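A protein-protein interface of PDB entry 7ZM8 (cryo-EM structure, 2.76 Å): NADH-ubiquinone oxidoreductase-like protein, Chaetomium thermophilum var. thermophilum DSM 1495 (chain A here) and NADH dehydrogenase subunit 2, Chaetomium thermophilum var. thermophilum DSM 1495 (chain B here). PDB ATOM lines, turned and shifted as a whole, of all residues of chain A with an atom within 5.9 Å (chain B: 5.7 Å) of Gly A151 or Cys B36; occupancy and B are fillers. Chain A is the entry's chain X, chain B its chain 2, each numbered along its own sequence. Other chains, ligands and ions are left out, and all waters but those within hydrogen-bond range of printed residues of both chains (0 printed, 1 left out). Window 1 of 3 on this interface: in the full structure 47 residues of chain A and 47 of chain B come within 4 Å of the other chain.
Gly A151 touches five residues of chain B.
Cys B36 touches one residue of chain A.
Printed residues of chain A within 4 Å of Met B1: Phe A150, Gly A151 and Val A152.
Printed residues of chain A within 4 Å of Asp B40: Gly A151.
Printed residues of chain B within 4 Å of Phe A150: Met B1.
Of the printed residues of chain A, His B39 touches Gln A92 (3.4 Å) and Gly A151 (3.7 Å).
Ala A147 touches none of the printed residues of chain B.
The nearest printed residue of chain A that does not touch Ile B2 is Phe A150 (4.9 Å).
O of His B39 lies within hydrogen-bond range of NE2 of Gln A92, at 3.4 Å.
The backbone carbonyl oxygen (O) of Phe A150 lies within hydrogen-bond range of the backbone NH (N) of Met B1 (2.8 Å).
O of Val A152 lies within hydrogen-bond range of N of Met B1, at 3.3 Å.
Along chain B the printed residues that touch a printed residue of chain A span positions 1 to 40.
Of the 8 printed residues of chain A, 4 touch a printed residue of chain B.
Printed residues of chain A that touch a printed residue of chain B: Gln A92, Phe A150, Gly A151 and Val A152.
Hydrophobic or aromatic side chains of chain A that line the printed part of chain B: Val A152.
Among the printed residues, 9 pairs touch across the chains.
Among the printed residues, no Asp or Glu carboxylate lies within 4 Å of a Lys or Arg side-chain nitrogen of the other chain.
NE2 of Gln A92 sits at hydrogen-bond distance from O of Ala A147, 2.7 Å away.
The backbone carbonyl oxygen of Met B1 sits at hydrogen-bond distance from the side-chain hydroxyl of Ser B5 (2.8 Å).
SG of Cys B36 lies within hydrogen-bond range of O of Ala B32, 3.3 Å away.
O of Tyr B35 lies within hydrogen-bond range of ND1 of His B39 (2.9 Å).
Among the printed residues, merely in contact across the chains: Gly A151 with Met B1 (3.8 Å), Gly A151 with Ile B2 (3.4 Å), Gly A151 with Cys B36 (3.8 Å), Gly A151 with His B39 (3.7 Å), Gly A151 with Asp B40 (3.96 Å) and Val A152 with Ile B2 (3.1 Å).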
ATOM      1  N   GLN A  92       8.239 -29.915  24.356  1.00  0.00           N
ATOM      2  CA  GLN A  92       7.116 -29.304  23.591  1.00  0.00           C
ATOM      3  C   GLN A  92       6.909 -29.994  22.245  1.00  0.00           C
ATOM      4  O   GLN A  92       5.776 -29.999  21.768  1.00  0.00           O
ATOM      5  CB  GLN A  92       7.375 -27.821  23.365  1.00  0.00           C
ATOM      6  CG  GLN A  92       6.411 -26.875  24.054  1.00  0.00           C
ATOM      7  CD  GLN A  92       6.768 -25.456  23.688  1.00  0.00           C
ATOM      8  OE1 GLN A  92       7.758 -25.210  23.007  1.00  0.00           O
ATOM      9  NE2 GLN A  92       5.957 -24.510  24.128  1.00  0.00           N
ATOM     10  N   ALA A 147       1.600 -26.851  27.837  1.00  0.00           N
ATOM     11  CA  ALA A 147       2.899 -26.693  27.178  1.00  0.00           C
ATOM     12  C   ALA A 147       2.746 -25.645  26.113  1.00  0.00           C
ATOM     13  O   ALA A 147       3.737 -25.242  25.520  1.00  0.00           O
ATOM     14  CB  ALA A 147       3.267 -27.988  26.572  1.00  0.00           C
ATOM     15  N   LEU A 148       1.510 -25.258  25.880  1.00  0.00           N
ATOM     16  CA  LEU A 148       1.330 -24.133  24.986  1.00  0.00           C
ATOM     17  C   LEU A 148       1.702 -22.815  25.631  1.00  0.00           C
ATOM     18  O   LEU A 148       1.499 -21.768  25.013  1.00  0.00           O
ATOM     19  CB  LEU A 148      -0.119 -24.081  24.509  1.00  0.00           C
ATOM     20  CG  LEU A 148      -0.580 -25.194  23.571  1.00  0.00           C
ATOM     21  CD1 LEU A 148      -2.092 -25.234  23.509  1.00  0.00           C
ATOM     22  CD2 LEU A 148       0.004 -24.987  22.202  1.00  0.00           C
ATOM     23  N   PHE A 149       2.239 -22.839  26.850  1.00  0.00           N
ATOM     24  CA  PHE A 149       2.583 -21.633  27.591  1.00  0.00           C
ATOM     25  C   PHE A 149       4.014 -21.669  28.130  1.00  0.00           C
ATOM     26  O   PHE A 149       4.355 -20.862  28.997  1.00  0.00           O
ATOM     27  CB  PHE A 149       1.574 -21.436  28.727  1.00  0.00           C
ATOM     28  CG  PHE A 149       1.422 -20.016  29.181  1.00  0.00           C
ATOM     29  CD1 PHE A 149       1.160 -19.004  28.273  1.00  0.00           C
ATOM     30  CD2 PHE A 149       1.523 -19.694  30.522  1.00  0.00           C
ATOM     31  CE1 PHE A 149       1.015 -17.701  28.693  1.00  0.00           C
ATOM     32  CE2 PHE A 149       1.383 -18.394  30.947  1.00  0.00           C
ATOM     33  CZ  PHE A 149       1.127 -17.398  30.030  1.00  0.00           C
ATOM     34  N   PHE A 150       4.870 -22.573  27.627  1.00  0.00           N
ATOM     35  CA  PHE A 150       6.240 -22.664  28.141  1.00  0.00           C
ATOM     36  C   PHE A 150       7.067 -21.417  27.883  1.00  0.00           C
ATOM     37  O   PHE A 150       7.987 -21.129  28.655  1.00  0.00           O
ATOM     38  CB  PHE A 150       6.991 -23.877  27.589  1.00  0.00           C
ATOM     39  CG  PHE A 150       6.492 -25.188  28.097  1.00  0.00           C
ATOM     40  CD1 PHE A 150       5.658 -25.237  29.191  1.00  0.00           C
ATOM     41  CD2 PHE A 150       6.947 -26.371  27.556  1.00  0.00           C
ATOM     42  CE1 PHE A 150       5.228 -26.427  29.689  1.00  0.00           C
ATOM     43  CE2 PHE A 150       6.524 -27.569  28.053  1.00  0.00           C
ATOM     44  CZ  PHE A 150       5.666 -27.601  29.127  1.00  0.00           C
ATOM     45  N   GLY A 151       6.785 -20.673  26.818  1.00  0.00           N
ATOM     46  CA  GLY A 151       7.533 -19.451  26.612  1.00  0.00           C
ATOM     47  C   GLY A 151       7.411 -18.479  27.764  1.00  0.00           C
ATOM     48  O   GLY A 151       8.233 -17.570  27.889  1.00  0.00           O
ATOM     49  N   VAL A 152       6.414 -18.667  28.625  1.00  0.00           N
ATOM     50  CA  VAL A 152       6.206 -17.828  29.802  1.00  0.00           C
ATOM     51  C   VAL A 152       6.462 -18.606  31.088  1.00  0.00           C
ATOM     52  O   VAL A 152       7.310 -18.227  31.894  1.00  0.00           O
ATOM     53  CB  VAL A 152       4.791 -17.207  29.798  1.00  0.00           C
ATOM     54  CG1 VAL A 152       4.561 -16.415  31.064  1.00  0.00           C
ATOM     55  CG2 VAL A 152       4.593 -16.334  28.574  1.00  0.00           C
ATOM     56  N   MET A 153       5.637 -19.636  31.286  1.00  0.00           N
ATOM     57  CA  MET A 153       5.681 -20.389  32.563  1.00  0.00           C
ATOM     58  C   MET A 153       5.841 -21.902  32.322  1.00  0.00           C
ATOM     59  O   MET A 153       5.074 -22.445  31.522  1.00  0.00           O
ATOM     60  CB  MET A 153       4.416 -20.114  33.383  1.00  0.00           C
ATOM     61  CG  MET A 153       4.468 -20.664  34.790  1.00  0.00           C
ATOM     62  SD  MET A 153       3.090 -20.059  35.786  1.00  0.00           S
ATOM     63  CE  MET A 153       1.753 -20.215  34.604  1.00  0.00           C
ATOM     64  N   MET B   1       9.665 -20.075  30.591  1.00  0.00           N
ATOM     65  CA  MET B   1      11.015 -19.812  30.119  1.00  0.00           C
ATOM     66  C   MET B   1      11.477 -18.428  30.566  1.00  0.00           C
ATOM     67  O   MET B   1      12.635 -18.254  30.935  1.00  0.00           O
ATOM     68  CB  MET B   1      11.095 -19.940  28.596  1.00  0.00           C
ATOM     69  CG  MET B   1      12.503 -19.811  28.037  1.00  0.00           C
ATOM     70  SD  MET B   1      13.605 -21.085  28.690  1.00  0.00           S
ATOM     71  CE  MET B   1      15.196 -20.273  28.570  1.00  0.00           C
ATOM     72  N   ILE B   2      10.576 -17.442  30.541  1.00  0.00           N
ATOM     73  CA  ILE B   2      10.930 -16.140  31.095  1.00  0.00           C
ATOM     74  C   ILE B   2      11.145 -16.251  32.597  1.00  0.00           C
ATOM     75  O   ILE B   2      11.977 -15.538  33.164  1.00  0.00           O
ATOM     76  CB  ILE B   2       9.874 -15.065  30.772  1.00  0.00           C
ATOM     77  CG1 ILE B   2       8.508 -15.457  31.306  1.00  0.00           C
ATOM     78  CG2 ILE B   2       9.751 -14.855  29.282  1.00  0.00           C
ATOM     79  CD1 ILE B   2       7.562 -14.313  31.389  1.00  0.00           C
ATOM     80  N   SER B   5      14.460 -18.018  33.216  1.00  0.00           N
ATOM     81  CA  SER B   5      15.541 -17.077  32.954  1.00  0.00           C
ATOM     82  C   SER B   5      15.700 -16.074  34.088  1.00  0.00           C
ATOM     83  O   SER B   5      16.824 -15.712  34.447  1.00  0.00           O
ATOM     84  CB  SER B   5      15.281 -16.356  31.640  1.00  0.00           C
ATOM     85  OG  SER B   5      15.226 -17.285  30.578  1.00  0.00           O
ATOM     86  N   ILE B  31      19.987 -13.985  24.734  1.00  0.00           N
ATOM     87  CA  ILE B  31      19.901 -15.406  24.419  1.00  0.00           C
ATOM     88  C   ILE B  31      18.700 -16.037  25.108  1.00  0.00           C
ATOM     89  O   ILE B  31      18.031 -16.910  24.543  1.00  0.00           O
ATOM     90  CB  ILE B  31      21.215 -16.111  24.803  1.00  0.00           C
ATOM     91  CG1 ILE B  31      22.352 -15.639  23.896  1.00  0.00           C
ATOM     92  CG2 ILE B  31      21.061 -17.616  24.734  1.00  0.00           C
ATOM     93  CD1 ILE B  31      23.719 -15.766  24.514  1.00  0.00           C
ATOM     94  N   ALA B  32      18.413 -15.618  26.340  1.00  0.00           N
ATOM     95  CA  ALA B  32      17.264 -16.155  27.057  1.00  0.00           C
ATOM     96  C   ALA B  32      15.960 -15.786  26.366  1.00  0.00           C
ATOM     97  O   ALA B  32      15.053 -16.618  26.249  1.00  0.00           O
ATOM     98  CB  ALA B  32      17.267 -15.657  28.498  1.00  0.00           C
ATOM     99  N   LEU B  33      15.844 -14.545  25.903  1.00  0.00           N
ATOM    100  CA  LEU B  33      14.636 -14.119  25.216  1.00  0.00           C
ATOM    101  C   LEU B  33      14.467 -14.805  23.872  1.00  0.00           C
ATOM    102  O   LEU B  33      13.347 -14.860  23.359  1.00  0.00           O
ATOM    103  CB  LEU B  33      14.649 -12.605  25.037  1.00  0.00           C
ATOM    104  CG  LEU B  33      14.131 -11.785  26.214  1.00  0.00           C
ATOM    105  CD1 LEU B  33      14.121 -10.325  25.854  1.00  0.00           C
ATOM    106  CD2 LEU B  33      12.749 -12.238  26.630  1.00  0.00           C
ATOM    107  N   ALA B  34      15.544 -15.329  23.294  1.00  0.00           N
ATOM    108  CA  ALA B  34      15.472 -16.055  22.007  1.00  0.00           C
ATOM    109  C   ALA B  34      14.856 -17.436  22.220  1.00  0.00           C
ATOM    110  O   ALA B  34      14.194 -17.917  21.306  1.00  0.00           O
ATOM    111  CB  ALA B  34      16.841 -16.142  21.408  1.00  0.00           C
ATOM    112  N   TYR B  35      15.076 -18.050  23.386  1.00  0.00           N
ATOM    113  CA  TYR B  35      14.422 -19.319  23.672  1.00  0.00           C
ATOM    114  C   TYR B  35      12.935 -19.128  23.912  1.00  0.00           C
ATOM    115  O   TYR B  35      12.136 -20.001  23.564  1.00  0.00           O
ATOM    116  CB  TYR B  35      15.069 -19.996  24.877  1.00  0.00           C
ATOM    117  CG  TYR B  35      16.319 -20.761  24.534  1.00  0.00           C
ATOM    118  CD1 TYR B  35      16.268 -21.893  23.739  1.00  0.00           C
ATOM    119  CD2 TYR B  35      17.554 -20.342  24.995  1.00  0.00           C
ATOM    120  CE1 TYR B  35      17.414 -22.581  23.419  1.00  0.00           C
ATOM    121  CE2 TYR B  35      18.697 -21.022  24.681  1.00  0.00           C
ATOM    122  CZ  TYR B  35      18.624 -22.136  23.895  1.00  0.00           C
ATOM    123  OH  TYR B  35      19.780 -22.800  23.592  1.00  0.00           O
ATOM    124  N   CYS B  36      12.551 -18.005  24.517  1.00  0.00           N
ATOM    125  CA  CYS B  36      11.139 -17.702  24.691  1.00  0.00           C
ATOM    126  C   CYS B  36      10.451 -17.534  23.346  1.00  0.00           C
ATOM    127  O   CYS B  36       9.315 -17.984  23.162  1.00  0.00           O
ATOM    128  CB  CYS B  36      10.974 -16.450  25.550  1.00  0.00           C
ATOM    129  SG  CYS B  36      11.908 -16.467  27.084  1.00  0.00           S
ATOM    130  N   ILE B  37      11.177 -16.985  22.375  1.00  0.00           N
ATOM    131  CA  ILE B  37      10.609 -16.810  21.011  1.00  0.00           C
ATOM    132  C   ILE B  37      10.404 -18.180  20.374  1.00  0.00           C
ATOM    133  O   ILE B  37       9.336 -18.392  19.811  1.00  0.00           O
ATOM    134  CB  ILE B  37      11.442 -15.842  20.143  1.00  0.00           C
ATOM    135  CG1 ILE B  37      11.267 -14.397  20.611  1.00  0.00           C
ATOM    136  CG2 ILE B  37      11.081 -15.979  18.674  1.00  0.00           C
ATOM    137  CD1 ILE B  37      12.378 -13.474  20.192  1.00  0.00           C
ATOM    138  N   LEU B  38      11.299 -19.117  20.627  1.00  0.00           N
ATOM    139  CA  LEU B  38      11.237 -20.444  19.987  1.00  0.00           C
ATOM    140  C   LEU B  38      10.164 -21.270  20.683  1.00  0.00           C
ATOM    141  O   LEU B  38       9.561 -22.114  20.026  1.00  0.00           O
ATOM    142  CB  LEU B  38      12.611 -21.091  20.181  1.00  0.00           C
ATOM    143  CG  LEU B  38      12.705 -22.598  19.939  1.00  0.00           C
ATOM    144  CD1 LEU B  38      12.553 -22.925  18.465  1.00  0.00           C
ATOM    145  CD2 LEU B  38      14.013 -23.153  20.468  1.00  0.00           C
ATOM    146  N   HIS B  39       9.898 -20.996  21.950  1.00  0.00           N
ATOM    147  CA  HIS B  39       8.818 -21.748  22.577  1.00  0.00           C
ATOM    148  C   HIS B  39       7.446 -21.215  22.186  1.00  0.00           C
ATOM    149  O   HIS B  39       6.537 -21.999  21.901  1.00  0.00           O
ATOM    150  CB  HIS B  39       8.991 -21.735  24.092  1.00  0.00           C
ATOM    151  CG  HIS B  39      10.204 -22.475  24.560  1.00  0.00           C
ATOM    152  ND1 HIS B  39      11.100 -21.943  25.459  1.00  0.00           N
ATOM    153  CD2 HIS B  39      10.676 -23.699  24.239  1.00  0.00           C
ATOM    154  CE1 HIS B  39      12.068 -22.812  25.676  1.00  0.00           C
ATOM    155  NE2 HIS B  39      11.837 -23.885  24.945  1.00  0.00           N
ATOM    156  N   ASP B  40       7.278 -19.893  22.163  1.00  0.00           N
ATOM    157  CA  ASP B  40       6.004 -19.320  21.752  1.00  0.00           C
ATOM    158  C   ASP B  40       5.750 -19.532  20.269  1.00  0.00           C
ATOM    159  O   ASP B  40       4.594 -19.591  19.841  1.00  0.00           O
ATOM    160  CB  ASP B  40       5.958 -17.832  22.097  1.00  0.00           C
ATOM    161  CG  ASP B  40       5.490 -17.576  23.516  1.00  0.00           C
ATOM    162  OD1 ASP B  40       4.711 -18.391  24.045  1.00  0.00           O
ATOM    163  OD2 ASP B  40       5.907 -16.564  24.113  1.00  0.00           O
ATOM    164  N   THR B  41       6.805 -19.673  19.465  1.00  0.00           N
ATOM    165  CA  THR B  41       6.661 -19.934  18.003  1.00  0.00           C
ATOM    166  C   THR B  41       6.034 -21.307  17.795  1.00  0.00           C
ATOM    167  O   THR B  41       5.251 -21.443  16.850  1.00  0.00           O
ATOM    168  CB  THR B  41       7.969 -19.669  17.242  1.00  0.00           C
ATOM    169  OG1 THR B  41       8.306 -18.292  17.410  1.00  0.00           O
ATOM    170  CG2 THR B  41       7.882 -19.932  15.759  1.00  0.00           C
ATOM    171  N   PHE B  72       8.909  -9.998  22.895  1.00  0.00           N
ATOM    172  CA  PHE B  72      10.249 -10.535  23.098  1.00  0.00           C
ATOM    173  C   PHE B  72      11.236  -9.981  22.078  1.00  0.00           C
ATOM    174  O   PHE B  72      12.403  -9.751  22.403  1.00  0.00           O
ATOM    175  CB  PHE B  72      10.219 -12.062  23.041  1.00  0.00           C
ATOM    176  CG  PHE B  72       9.426 -12.695  24.142  1.00  0.00           C
ATOM    177  CD1 PHE B  72       9.275 -12.055  25.356  1.00  0.00           C
ATOM    178  CD2 PHE B  72       8.823 -13.928  23.961  1.00  0.00           C
ATOM    179  CE1 PHE B  72       8.538 -12.632  26.366  1.00  0.00           C
ATOM    180  CE2 PHE B  72       8.086 -14.511  24.971  1.00  0.00           C
ATOM    181  CZ  PHE B  72       7.943 -13.861  26.174  1.00  0.00           C
